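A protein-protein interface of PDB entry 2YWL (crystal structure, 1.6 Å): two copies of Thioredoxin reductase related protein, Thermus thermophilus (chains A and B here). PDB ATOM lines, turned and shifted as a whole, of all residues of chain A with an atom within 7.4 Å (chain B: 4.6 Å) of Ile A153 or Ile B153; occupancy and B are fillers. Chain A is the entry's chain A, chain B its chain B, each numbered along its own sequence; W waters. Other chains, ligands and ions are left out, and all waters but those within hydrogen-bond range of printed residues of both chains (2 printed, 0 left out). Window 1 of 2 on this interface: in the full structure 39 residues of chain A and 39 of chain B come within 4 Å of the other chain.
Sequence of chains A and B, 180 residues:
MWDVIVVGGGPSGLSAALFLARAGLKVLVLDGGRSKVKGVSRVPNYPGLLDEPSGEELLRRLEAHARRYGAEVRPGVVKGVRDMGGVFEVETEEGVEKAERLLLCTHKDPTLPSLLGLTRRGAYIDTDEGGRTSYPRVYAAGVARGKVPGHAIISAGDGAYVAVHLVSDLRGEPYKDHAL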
ATOM      1  N   PRO A  11      14.810 -23.000   3.565  1.00  0.00           N
ATOM      2  CA  PRO A  11      14.914 -22.227   2.323  1.00  0.00           C
ATOM      3  C   PRO A  11      14.674 -23.025   1.035  1.00  0.00           C
ATOM      4  O   PRO A  11      14.018 -22.532   0.113  1.00  0.00           O
ATOM      5  CB  PRO A  11      16.321 -21.643   2.403  1.00  0.00           C
ATOM      6  CG  PRO A  11      16.495 -21.437   3.883  1.00  0.00           C
ATOM      7  CD  PRO A  11      15.962 -22.733   4.445  1.00  0.00           C
ATOM      8  N   SER A  15      11.211 -22.279  -1.094  1.00  0.00           N
ATOM      9  CA  SER A  15      11.466 -21.725  -2.419  1.00  0.00           C
ATOM     10  C   SER A  15      10.814 -22.628  -3.467  1.00  0.00           C
ATOM     11  O   SER A  15      10.173 -22.154  -4.403  1.00  0.00           O
ATOM     12  CB  SER A  15      12.970 -21.623  -2.679  1.00  0.00           C
ATOM     13  OG  SER A  15      13.206 -21.139  -3.990  1.00  0.00           O
ATOM     14  N   LEU A  18       7.077 -22.072  -3.571  1.00  0.00           N
ATOM     15  CA  LEU A  18       6.712 -20.846  -4.268  1.00  0.00           C
ATOM     16  C   LEU A  18       6.644 -21.106  -5.772  1.00  0.00           C
ATOM     17  O   LEU A  18       5.660 -20.760  -6.429  1.00  0.00           O
ATOM     18  CB  LEU A  18       7.744 -19.749  -3.986  1.00  0.00           C
ATOM     19  CG  LEU A  18       7.669 -18.497  -4.866  1.00  0.00           C
ATOM     20  CD1 LEU A  18       6.313 -17.829  -4.712  1.00  0.00           C
ATOM     21  CD2 LEU A  18       8.780 -17.538  -4.470  1.00  0.00           C
ATOM     22  N   PHE A  19       7.688 -21.722  -6.315  1.00  0.00           N
ATOM     23  CA  PHE A  19       7.716 -22.000  -7.746  1.00  0.00           C
ATOM     24  C   PHE A  19       6.660 -22.995  -8.196  1.00  0.00           C
ATOM     25  O   PHE A  19       6.041 -22.816  -9.249  1.00  0.00           O
ATOM     26  CB  PHE A  19       9.115 -22.462  -8.174  1.00  0.00           C
ATOM     27  CG  PHE A  19      10.049 -21.323  -8.474  1.00  0.00           C
ATOM     28  CD1 PHE A  19      10.507 -20.494  -7.453  1.00  0.00           C
ATOM     29  CD2 PHE A  19      10.409 -21.030  -9.788  1.00  0.00           C
ATOM     30  CE1 PHE A  19      11.306 -19.385  -7.736  1.00  0.00           C
ATOM     31  CE2 PHE A  19      11.205 -19.924 -10.082  1.00  0.00           C
ATOM     32  CZ  PHE A  19      11.655 -19.099  -9.050  1.00  0.00           C
ATOM     33  N   VAL A  43      21.001 -12.924   9.197  1.00  0.00           N
ATOM     34  CA  VAL A  43      21.512 -13.554   7.978  1.00  0.00           C
ATOM     35  C   VAL A  43      21.969 -12.394   7.096  1.00  0.00           C
ATOM     36  O   VAL A  43      21.152 -11.684   6.511  1.00  0.00           O
ATOM     37  CB  VAL A  43      20.404 -14.361   7.248  1.00  0.00           C
ATOM     38  CG1 VAL A  43      20.985 -15.057   6.029  1.00  0.00           C
ATOM     39  CG2 VAL A  43      19.792 -15.382   8.197  1.00  0.00           C
ATOM     40  N   ASN A  45      24.039 -12.727   4.391  1.00  0.00           N
ATOM     41  CA  ASN A  45      24.445 -13.179   3.070  1.00  0.00           C
ATOM     42  C   ASN A  45      23.389 -13.830   2.179  1.00  0.00           C
ATOM     43  O   ASN A  45      23.682 -14.789   1.467  1.00  0.00           O
ATOM     44  CB  ASN A  45      25.662 -14.106   3.202  1.00  0.00           C
ATOM     45  CG  ASN A  45      25.421 -15.265   4.154  1.00  0.00           C
ATOM     46  OD1 ASN A  45      24.358 -15.375   4.762  1.00  0.00           O
ATOM     47  ND2 ASN A  45      26.415 -16.131   4.291  1.00  0.00           N
ATOM     48  N   TYR A  46      22.164 -13.319   2.232  1.00  0.00           N
ATOM     49  CA  TYR A  46      21.100 -13.804   1.359  1.00  0.00           C
ATOM     50  C   TYR A  46      21.002 -12.622   0.393  1.00  0.00           C
ATOM     51  O   TYR A  46      20.306 -11.645   0.666  1.00  0.00           O
ATOM     52  CB  TYR A  46      19.784 -13.977   2.125  1.00  0.00           C
ATOM     53  CG  TYR A  46      18.698 -14.708   1.353  1.00  0.00           C
ATOM     54  CD1 TYR A  46      18.570 -16.096   1.426  1.00  0.00           C
ATOM     55  CD2 TYR A  46      17.796 -14.009   0.549  1.00  0.00           C
ATOM     56  CE1 TYR A  46      17.568 -16.768   0.721  1.00  0.00           C
ATOM     57  CE2 TYR A  46      16.790 -14.676  -0.164  1.00  0.00           C
ATOM     58  CZ  TYR A  46      16.683 -16.054  -0.069  1.00  0.00           C
ATOM     59  OH  TYR A  46      15.679 -16.718  -0.749  1.00  0.00           O
ATOM     60  N   PRO A  47      21.715 -12.691  -0.742  1.00  0.00           N
ATOM     61  CA  PRO A  47      21.728 -11.622  -1.748  1.00  0.00           C
ATOM     62  C   PRO A  47      20.394 -10.933  -2.004  1.00  0.00           C
ATOM     63  O   PRO A  47      19.429 -11.563  -2.434  1.00  0.00           O
ATOM     64  CB  PRO A  47      22.265 -12.322  -2.993  1.00  0.00           C
ATOM     65  CG  PRO A  47      23.163 -13.371  -2.427  1.00  0.00           C
ATOM     66  CD  PRO A  47      22.351 -13.910  -1.273  1.00  0.00           C
ATOM     67  N   GLY A  48      20.347  -9.631  -1.740  1.00  0.00           N
ATOM     68  CA  GLY A  48      19.122  -8.887  -1.967  1.00  0.00           C
ATOM     69  C   GLY A  48      18.341  -8.538  -0.716  1.00  0.00           C
ATOM     70  O   GLY A  48      17.577  -7.571  -0.716  1.00  0.00           O
ATOM     71  N   LEU A  58      13.488 -14.692   8.040  1.00  0.00           N
ATOM     72  CA  LEU A  58      13.687 -15.113   6.659  1.00  0.00           C
ATOM     73  C   LEU A  58      12.676 -16.204   6.312  1.00  0.00           C
ATOM     74  O   LEU A  58      12.012 -16.145   5.274  1.00  0.00           O
ATOM     75  CB  LEU A  58      15.107 -15.646   6.460  1.00  0.00           C
ATOM     76  CG  LEU A  58      15.408 -16.245   5.083  1.00  0.00           C
ATOM     77  CD1 LEU A  58      15.111 -15.229   3.994  1.00  0.00           C
ATOM     78  CD2 LEU A  58      16.867 -16.686   5.029  1.00  0.00           C
ATOM     79  N   LEU A  62       9.660 -16.199   3.543  1.00  0.00           N
ATOM     80  CA  LEU A  62       9.608 -17.232   2.511  1.00  0.00           C
ATOM     81  C   LEU A  62       8.253 -17.929   2.523  1.00  0.00           C
ATOM     82  O   LEU A  62       7.687 -18.217   1.470  1.00  0.00           O
ATOM     83  CB  LEU A  62      10.721 -18.257   2.724  1.00  0.00           C
ATOM     84  CG  LEU A  62      12.135 -17.746   2.460  1.00  0.00           C
ATOM     85  CD1 LEU A  62      13.156 -18.799   2.858  1.00  0.00           C
ATOM     86  CD2 LEU A  62      12.268 -17.388   0.999  1.00  0.00           C
ATOM     87  N   GLY A 150      26.213 -25.962   3.250  1.00  0.00           N
ATOM     88  CA  GLY A 150      24.929 -25.308   3.097  1.00  0.00           C
ATOM     89  C   GLY A 150      24.828 -23.833   3.443  1.00  0.00           C
ATOM     90  O   GLY A 150      25.430 -23.356   4.405  1.00  0.00           O
ATOM     91  N   HIS A 151      24.061 -23.111   2.628  1.00  0.00           N
ATOM     92  CA  HIS A 151      23.782 -21.693   2.841  1.00  0.00           C
ATOM     93  C   HIS A 151      22.350 -21.456   2.374  1.00  0.00           C
ATOM     94  O   HIS A 151      21.868 -22.129   1.463  1.00  0.00           O
ATOM     95  CB  HIS A 151      24.755 -20.795   2.071  1.00  0.00           C
ATOM     96  CG  HIS A 151      26.160 -20.861   2.582  1.00  0.00           C
ATOM     97  ND1 HIS A 151      27.014 -21.899   2.276  1.00  0.00           N
ATOM     98  CD2 HIS A 151      26.840 -20.052   3.429  1.00  0.00           C
ATOM     99  CE1 HIS A 151      28.158 -21.728   2.915  1.00  0.00           C
ATOM    100  NE2 HIS A 151      28.078 -20.615   3.623  1.00  0.00           N
ATOM    101  N   ALA A 152      21.672 -20.508   3.009  1.00  0.00           N
ATOM    102  CA  ALA A 152      20.280 -20.207   2.689  1.00  0.00           C
ATOM    103  C   ALA A 152      20.003 -19.917   1.217  1.00  0.00           C
ATOM    104  O   ALA A 152      19.092 -20.501   0.628  1.00  0.00           O
ATOM    105  CB  ALA A 152      19.794 -19.043   3.546  1.00  0.00           C
ATOM    106  N   ILE A 153      20.779 -19.018   0.620  1.00  0.00           N
ATOM    107  CA  ILE A 153      20.558 -18.674  -0.783  1.00  0.00           C
ATOM    108  C   ILE A 153      20.850 -19.856  -1.717  1.00  0.00           C
ATOM    109  O   ILE A 153      20.191 -20.015  -2.744  1.00  0.00           O
ATOM    110  CB  ILE A 153      21.414 -17.440  -1.206  1.00  0.00           C
ATOM    111  CG1 ILE A 153      20.981 -16.955  -2.591  1.00  0.00           C
ATOM    112  CG2 ILE A 153      22.897 -17.783  -1.178  1.00  0.00           C
ATOM    113  CD1 ILE A 153      19.622 -16.288  -2.599  1.00  0.00           C
ATOM    114  N   ILE A 154      21.828 -20.686  -1.354  1.00  0.00           N
ATOM    115  CA  ILE A 154      22.181 -21.852  -2.165  1.00  0.00           C
ATOM    116  C   ILE A 154      21.015 -22.836  -2.165  1.00  0.00           C
ATOM    117  O   ILE A 154      20.634 -23.358  -3.213  1.00  0.00           O
ATOM    118  CB  ILE A 154      23.443 -22.559  -1.615  1.00  0.00           C
ATOM    119  CG1 ILE A 154      24.647 -21.616  -1.724  1.00  0.00           C
ATOM    120  CG2 ILE A 154      23.705 -23.846  -2.385  1.00  0.00           C
ATOM    121  CD1 ILE A 154      25.935 -22.198  -1.159  1.00  0.00           C
ATOM    122  N   SER A 155      20.443 -23.077  -0.988  1.00  0.00           N
ATOM    123  CA  SER A 155      19.312 -23.989  -0.881  1.00  0.00           C
ATOM    124  C   SER A 155      18.056 -23.419  -1.529  1.00  0.00           C
ATOM    125  O   SER A 155      17.307 -24.154  -2.163  1.00  0.00           O
ATOM    126  CB  SER A 155      19.040 -24.343   0.587  1.00  0.00           C
ATOM    127  OG  SER A 155      19.925 -25.369   1.011  1.00  0.00           O
ATOM    128  N   ALA A 156      17.829 -22.117  -1.385  1.00  0.00           N
ATOM    129  CA  ALA A 156      16.650 -21.496  -1.992  1.00  0.00           C
ATOM    130  C   ALA A 156      16.750 -21.606  -3.511  1.00  0.00           C
ATOM    131  O   ALA A 156      15.774 -21.931  -4.190  1.00  0.00           O
ATOM    132  CB  ALA A 156      16.551 -20.031  -1.578  1.00  0.00           C
ATOM    133  N   GLY A 157      17.940 -21.330  -4.040  1.00  0.00           N
ATOM    134  CA  GLY A 157      18.142 -21.414  -5.474  1.00  0.00           C
ATOM    135  C   GLY A 157      17.965 -22.830  -5.987  1.00  0.00           C
ATOM    136  O   GLY A 157      17.339 -23.048  -7.026  1.00  0.00           O
ATOM    137  N   ASP A 158      18.497 -23.809  -5.261  1.00  0.00           N
ATOM    138  CA  ASP A 158      18.371 -25.186  -5.716  1.00  0.00           C
ATOM    139  C   ASP A 158      16.934 -25.683  -5.612  1.00  0.00           C
ATOM    140  O   ASP A 158      16.489 -26.478  -6.442  1.00  0.00           O
ATOM    141  CB  ASP A 158      19.317 -26.107  -4.939  1.00  0.00           C
ATOM    142  CG  ASP A 158      19.550 -27.417  -5.655  1.00  0.00           C
ATOM    143  OD1 ASP A 158      19.955 -27.374  -6.838  1.00  0.00           O
ATOM    144  OD2 ASP A 158      19.329 -28.483  -5.046  1.00  0.00           O
ATOM    145  N   GLY A 159      16.207 -25.218  -4.600  1.00  0.00           N
ATOM    146  CA  GLY A 159      14.821 -25.622  -4.454  1.00  0.00           C
ATOM    147  C   GLY A 159      14.022 -25.168  -5.665  1.00  0.00           C
ATOM    148  O   GLY A 159      13.200 -25.912  -6.187  1.00  0.00           O
ATOM    149  N   ALA A 160      14.271 -23.942  -6.114  1.00  0.00           N
ATOM    150  CA  ALA A 160      13.568 -23.408  -7.278  1.00  0.00           C
ATOM    151  C   ALA A 160      13.978 -24.156  -8.545  1.00  0.00           C
ATOM    152  O   ALA A 160      13.146 -24.440  -9.406  1.00  0.00           O
ATOM    153  CB  ALA A 160      13.867 -21.915  -7.435  1.00  0.00           C
ATOM    154  N   TYR A 161      15.266 -24.470  -8.651  1.00  0.00           N
ATOM    155  CA  TYR A 161      15.806 -25.174  -9.810  1.00  0.00           C
ATOM    156  C   TYR A 161      15.174 -26.553  -9.984  1.00  0.00           C
ATOM    157  O   TYR A 161      14.764 -26.927 -11.086  1.00  0.00           O
ATOM    158  CB  TYR A 161      17.323 -25.305  -9.660  1.00  0.00           C
ATOM    159  CG  TYR A 161      18.039 -25.929 -10.841  1.00  0.00           C
ATOM    160  CD1 TYR A 161      17.896 -25.410 -12.131  1.00  0.00           C
ATOM    161  CD2 TYR A 161      18.903 -27.007 -10.658  1.00  0.00           C
ATOM    162  CE1 TYR A 161      18.604 -25.952 -13.208  1.00  0.00           C
ATOM    163  CE2 TYR A 161      19.613 -27.553 -11.722  1.00  0.00           C
ATOM    164  CZ  TYR A 161      19.461 -27.020 -12.994  1.00  0.00           C
ATOM    165  OH  TYR A 161      20.181 -27.551 -14.042  1.00  0.00           O
ATOM    166  N   PHE B  19      29.640 -13.225  -1.655  1.00  0.00           N
ATOM    167  CA  PHE B  19      30.281 -14.278  -0.877  1.00  0.00           C
ATOM    168  C   PHE B  19      31.799 -14.198  -0.897  1.00  0.00           C
ATOM    169  O   PHE B  19      32.452 -14.424   0.121  1.00  0.00           O
ATOM    170  CB  PHE B  19      29.815 -15.658  -1.358  1.00  0.00           C
ATOM    171  CG  PHE B  19      28.519 -16.098  -0.741  1.00  0.00           C
ATOM    172  CD1 PHE B  19      27.322 -15.488  -1.097  1.00  0.00           C
ATOM    173  CD2 PHE B  19      28.504 -17.079   0.250  1.00  0.00           C
ATOM    174  CE1 PHE B  19      26.129 -15.841  -0.475  1.00  0.00           C
ATOM    175  CE2 PHE B  19      27.312 -17.441   0.880  1.00  0.00           C
ATOM    176  CZ  PHE B  19      26.121 -16.818   0.517  1.00  0.00           C
ATOM    177  N   ASN B  45       9.075 -13.703  -8.154  1.00  0.00           N
ATOM    178  CA  ASN B  45       9.550 -14.987  -7.682  1.00  0.00           C
ATOM    179  C   ASN B  45      10.975 -15.085  -7.158  1.00  0.00           C
ATOM    180  O   ASN B  45      11.668 -16.061  -7.430  1.00  0.00           O
ATOM    181  CB  ASN B  45       9.330 -16.036  -8.778  1.00  0.00           C
ATOM    182  CG  ASN B  45       9.966 -15.651 -10.099  1.00  0.00           C
ATOM    183  OD1 ASN B  45      10.532 -14.565 -10.242  1.00  0.00           O
ATOM    184  ND2 ASN B  45       9.873 -16.546 -11.079  1.00  0.00           N
ATOM    185  N   TYR B  46      11.422 -14.073  -6.423  1.00  0.00           N
ATOM    186  CA  TYR B  46      12.748 -14.127  -5.813  1.00  0.00           C
ATOM    187  C   TYR B  46      12.367 -14.351  -4.350  1.00  0.00           C
ATOM    188  O   TYR B  46      12.048 -13.407  -3.625  1.00  0.00           O
ATOM    189  CB  TYR B  46      13.503 -12.804  -5.985  1.00  0.00           C
ATOM    190  CG  TYR B  46      14.974 -12.892  -5.630  1.00  0.00           C
ATOM    191  CD1 TYR B  46      15.925 -13.265  -6.582  1.00  0.00           C
ATOM    192  CD2 TYR B  46      15.416 -12.609  -4.336  1.00  0.00           C
ATOM    193  CE1 TYR B  46      17.286 -13.350  -6.254  1.00  0.00           C
ATOM    194  CE2 TYR B  46      16.773 -12.691  -3.999  1.00  0.00           C
ATOM    195  CZ  TYR B  46      17.699 -13.059  -4.964  1.00  0.00           C
ATOM    196  OH  TYR B  46      19.037 -13.109  -4.635  1.00  0.00           O
ATOM    197  N   PRO B  47      12.376 -15.617  -3.905  1.00  0.00           N
ATOM    198  CA  PRO B  47      12.020 -16.011  -2.538  1.00  0.00           C
ATOM    199  C   PRO B  47      12.465 -15.078  -1.421  1.00  0.00           C
ATOM    200  O   PRO B  47      13.657 -14.926  -1.159  1.00  0.00           O
ATOM    201  CB  PRO B  47      12.630 -17.401  -2.411  1.00  0.00           C
ATOM    202  CG  PRO B  47      12.513 -17.936  -3.810  1.00  0.00           C
ATOM    203  CD  PRO B  47      12.955 -16.758  -4.640  1.00  0.00           C
ATOM    204  N   HIS B 151      16.568 -18.420 -13.931  1.00  0.00           N
ATOM    205  CA  HIS B 151      15.747 -17.629 -13.017  1.00  0.00           C
ATOM    206  C   HIS B 151      16.711 -16.909 -12.074  1.00  0.00           C
ATOM    207  O   HIS B 151      17.798 -17.408 -11.784  1.00  0.00           O
ATOM    208  CB  HIS B 151      14.765 -18.513 -12.235  1.00  0.00           C
ATOM    209  CG  HIS B 151      13.686 -19.106 -13.089  1.00  0.00           C
ATOM    210  ND1 HIS B 151      13.883 -20.224 -13.869  1.00  0.00           N
ATOM    211  CD2 HIS B 151      12.415 -18.700 -13.327  1.00  0.00           C
ATOM    212  CE1 HIS B 151      12.781 -20.484 -14.551  1.00  0.00           C
ATOM    213  NE2 HIS B 151      11.876 -19.573 -14.241  1.00  0.00           N
ATOM    214  N   ALA B 152      16.321 -15.728 -11.614  1.00  0.00           N
ATOM    215  CA  ALA B 152      17.176 -14.933 -10.741  1.00  0.00           C
ATOM    216  C   ALA B 152      17.649 -15.647  -9.482  1.00  0.00           C
ATOM    217  O   ALA B 152      18.839 -15.619  -9.158  1.00  0.00           O
ATOM    218  CB  ALA B 152      16.469 -13.636 -10.371  1.00  0.00           C
ATOM    219  N   ILE B 153      16.732 -16.287  -8.765  1.00  0.00           N
ATOM    220  CA  ILE B 153      17.122 -16.976  -7.540  1.00  0.00           C
ATOM    221  C   ILE B 153      18.024 -18.176  -7.824  1.00  0.00           C
ATOM    222  O   ILE B 153      18.928 -18.481  -7.040  1.00  0.00           O
ATOM    223  CB  ILE B 153      15.884 -17.447  -6.732  1.00  0.00           C
ATOM    224  CG1 ILE B 153      16.324 -17.933  -5.350  1.00  0.00           C
ATOM    225  CG2 ILE B 153      15.142 -18.537  -7.481  1.00  0.00           C
ATOM    226  CD1 ILE B 153      16.840 -16.817  -4.459  1.00  0.00           C
ATOM    227  N   ILE B 154      17.780 -18.853  -8.941  1.00  0.00           N
ATOM    228  CA  ILE B 154      18.588 -20.008  -9.322  1.00  0.00           C
ATOM    229  C   ILE B 154      20.022 -19.562  -9.595  1.00  0.00           C
ATOM    230  O   ILE B 154      20.978 -20.180  -9.118  1.00  0.00           O
ATOM    231  CB  ILE B 154      18.013 -20.703 -10.584  1.00  0.00           C
ATOM    232  CG1 ILE B 154      16.617 -21.260 -10.272  1.00  0.00           C
ATOM    233  CG2 ILE B 154      18.947 -21.820 -11.040  1.00  0.00           C
ATOM    234  CD1 ILE B 154      15.920 -21.925 -11.459  1.00  0.00           C
ATOM    235  N   SER B 155      20.178 -18.482 -10.355  1.00  0.00           N
ATOM    236  CA  SER B 155      21.512 -17.974 -10.652  1.00  0.00           C
ATOM    237  C   SER B 155      22.185 -17.382  -9.415  1.00  0.00           C
ATOM    238  O   SER B 155      23.390 -17.539  -9.234  1.00  0.00           O
ATOM    239  CB  SER B 155      21.454 -16.939 -11.772  1.00  0.00           C
ATOM    240  OG  SER B 155      21.342 -17.582 -13.029  1.00  0.00           O
ATOM    241  N   ALA B 156      21.416 -16.709  -8.563  1.00  0.00           N
ATOM    242  CA  ALA B 156      21.989 -16.135  -7.346  1.00  0.00           C
ATOM    243  C   ALA B 156      22.493 -17.269  -6.458  1.00  0.00           C
ATOM    244  O   ALA B 156      23.597 -17.213  -5.912  1.00  0.00           O
ATOM    245  CB  ALA B 156      20.941 -15.311  -6.600  1.00  0.00           C
ATOM    246  N   GLY B 157      21.680 -18.309  -6.315  1.00  0.00           N
ATOM    247  CA  GLY B 157      22.092 -19.431  -5.495  1.00  0.00           C
ATOM    248  C   GLY B 157      23.318 -20.133  -6.045  1.00  0.00           C
ATOM    249  O   GLY B 157      24.224 -20.498  -5.293  1.00  0.00           O
ATOM    250  N   ALA B 160      26.563 -18.188  -5.477  1.00  0.00           N
ATOM    251  CA  ALA B 160      27.049 -18.338  -4.110  1.00  0.00           C
ATOM    252  C   ALA B 160      27.696 -19.707  -3.925  1.00  0.00           C
ATOM    253  O   ALA B 160      28.737 -19.835  -3.277  1.00  0.00           O
ATOM    254  CB  ALA B 160      25.892 -18.166  -3.122  1.00  0.00           C
HETATM  255  O   HOH W   1      22.074 -23.046  -5.592  1.00  0.00           O
HETATM  256  O   HOH W   2      20.581 -22.693  -7.847  1.00  0.00           O
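The backbone carbonyl oxygen (O) of Pro A47 lies within hydrogen-bond range of the side-chain hydroxyl (OH) of Tyr B46, at 2.7 Å.
The side-chain hydroxyl (OH) of Tyr A46 sits at hydrogen-bond distance from the backbone carbonyl oxygen (O) of Pro B47 (2.7 Å).
OG of Ser A15 lies within hydrogen-bond range of O of Ala A156 (2.7 Å).
Ser A15 touches Pro B47.
Phe A19 touches Ile B153 (CZ to CG2, 3.9 Å).
CE1 of Phe B19 touches O of Asn A45, 3.3 Å away.
OH of Tyr A46 touches CD1 of Ile B153 (3.9 Å).
CD2 of His A151 touches CE2 of Phe B19 (3.7 Å).
Ile A153 touches Ile B153 (CD1 to CD1, 3.4 Å).
O of Ile A153 touches CA of Gly B157, 3.4 Å away.
Ile A153 touches Ala B160 (CG2 to CB, 3.6 Å).
CG1 of Ile A154 touches CB of Ala B160, at 3.9 Å.
Ile B154 touches Gly A157.
Of chain A, only Phe A19, Tyr A46, Ile A153, Gly A157 and Ala A160 come within 4 Å of Ile B153.
No residue of chain A comes within 4 Å of Ala B152.
Of the printed residues of chain B, Phe A19 touches Asn B45 (3.4 Å), His B151 (3.7 Å) and Ile B153 (3.9 Å).
Printed residues of chain B within 4 Å of Tyr A161: Ile B154.
Pro A11 touches none of the printed residues of chain B.
The nearest residue of chain B that does not touch Ile A153 is Ala B156 (4.2 Å).
The nearest residue of chain A that does not touch Ile B153 is Ala A156 (4.1 Å).
Of the 23 printed residues of chain A, 13 touch a printed residue of chain B.
Of the 12 printed residues of chain B, 9 touch a printed residue of chain A.
Hydrophobic or aromatic side chains of chain B within 4 Å of the printed part of chain A: Phe B19, Tyr B46, Pro B47, His B151, Ile B153, Ile B154 and Ala B160.
Tyr A46 touches Ile B153, and with the chains exchanged Ile A153 touches Tyr B46.
Ile B153 touches its own counterpart, Ile A153.
Ile A153 touches Ala B160, and with the chains exchanged Ala A160 touches Ile B153.
Ile A154 touches Ala B160, but with the chains exchanged Ala A160 does not touch Ile B154 (4.01 Å).
Positions printed for both chains: 19, 45, 46, 47, 151, 152, 153, 154, 155, 156, 157 and 160.
Of the 22 pairs that touch across the chains among the printed residues, 17 have their exchanged pair printed and touching as well.
Water W1 lies within hydrogen-bond range of O of Ile A154 and O of Gly B157.
Water W2 lies within hydrogen-bond range of O of Ile B154 (2.8 Å) and O of Gly A157 (3.4 Å).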
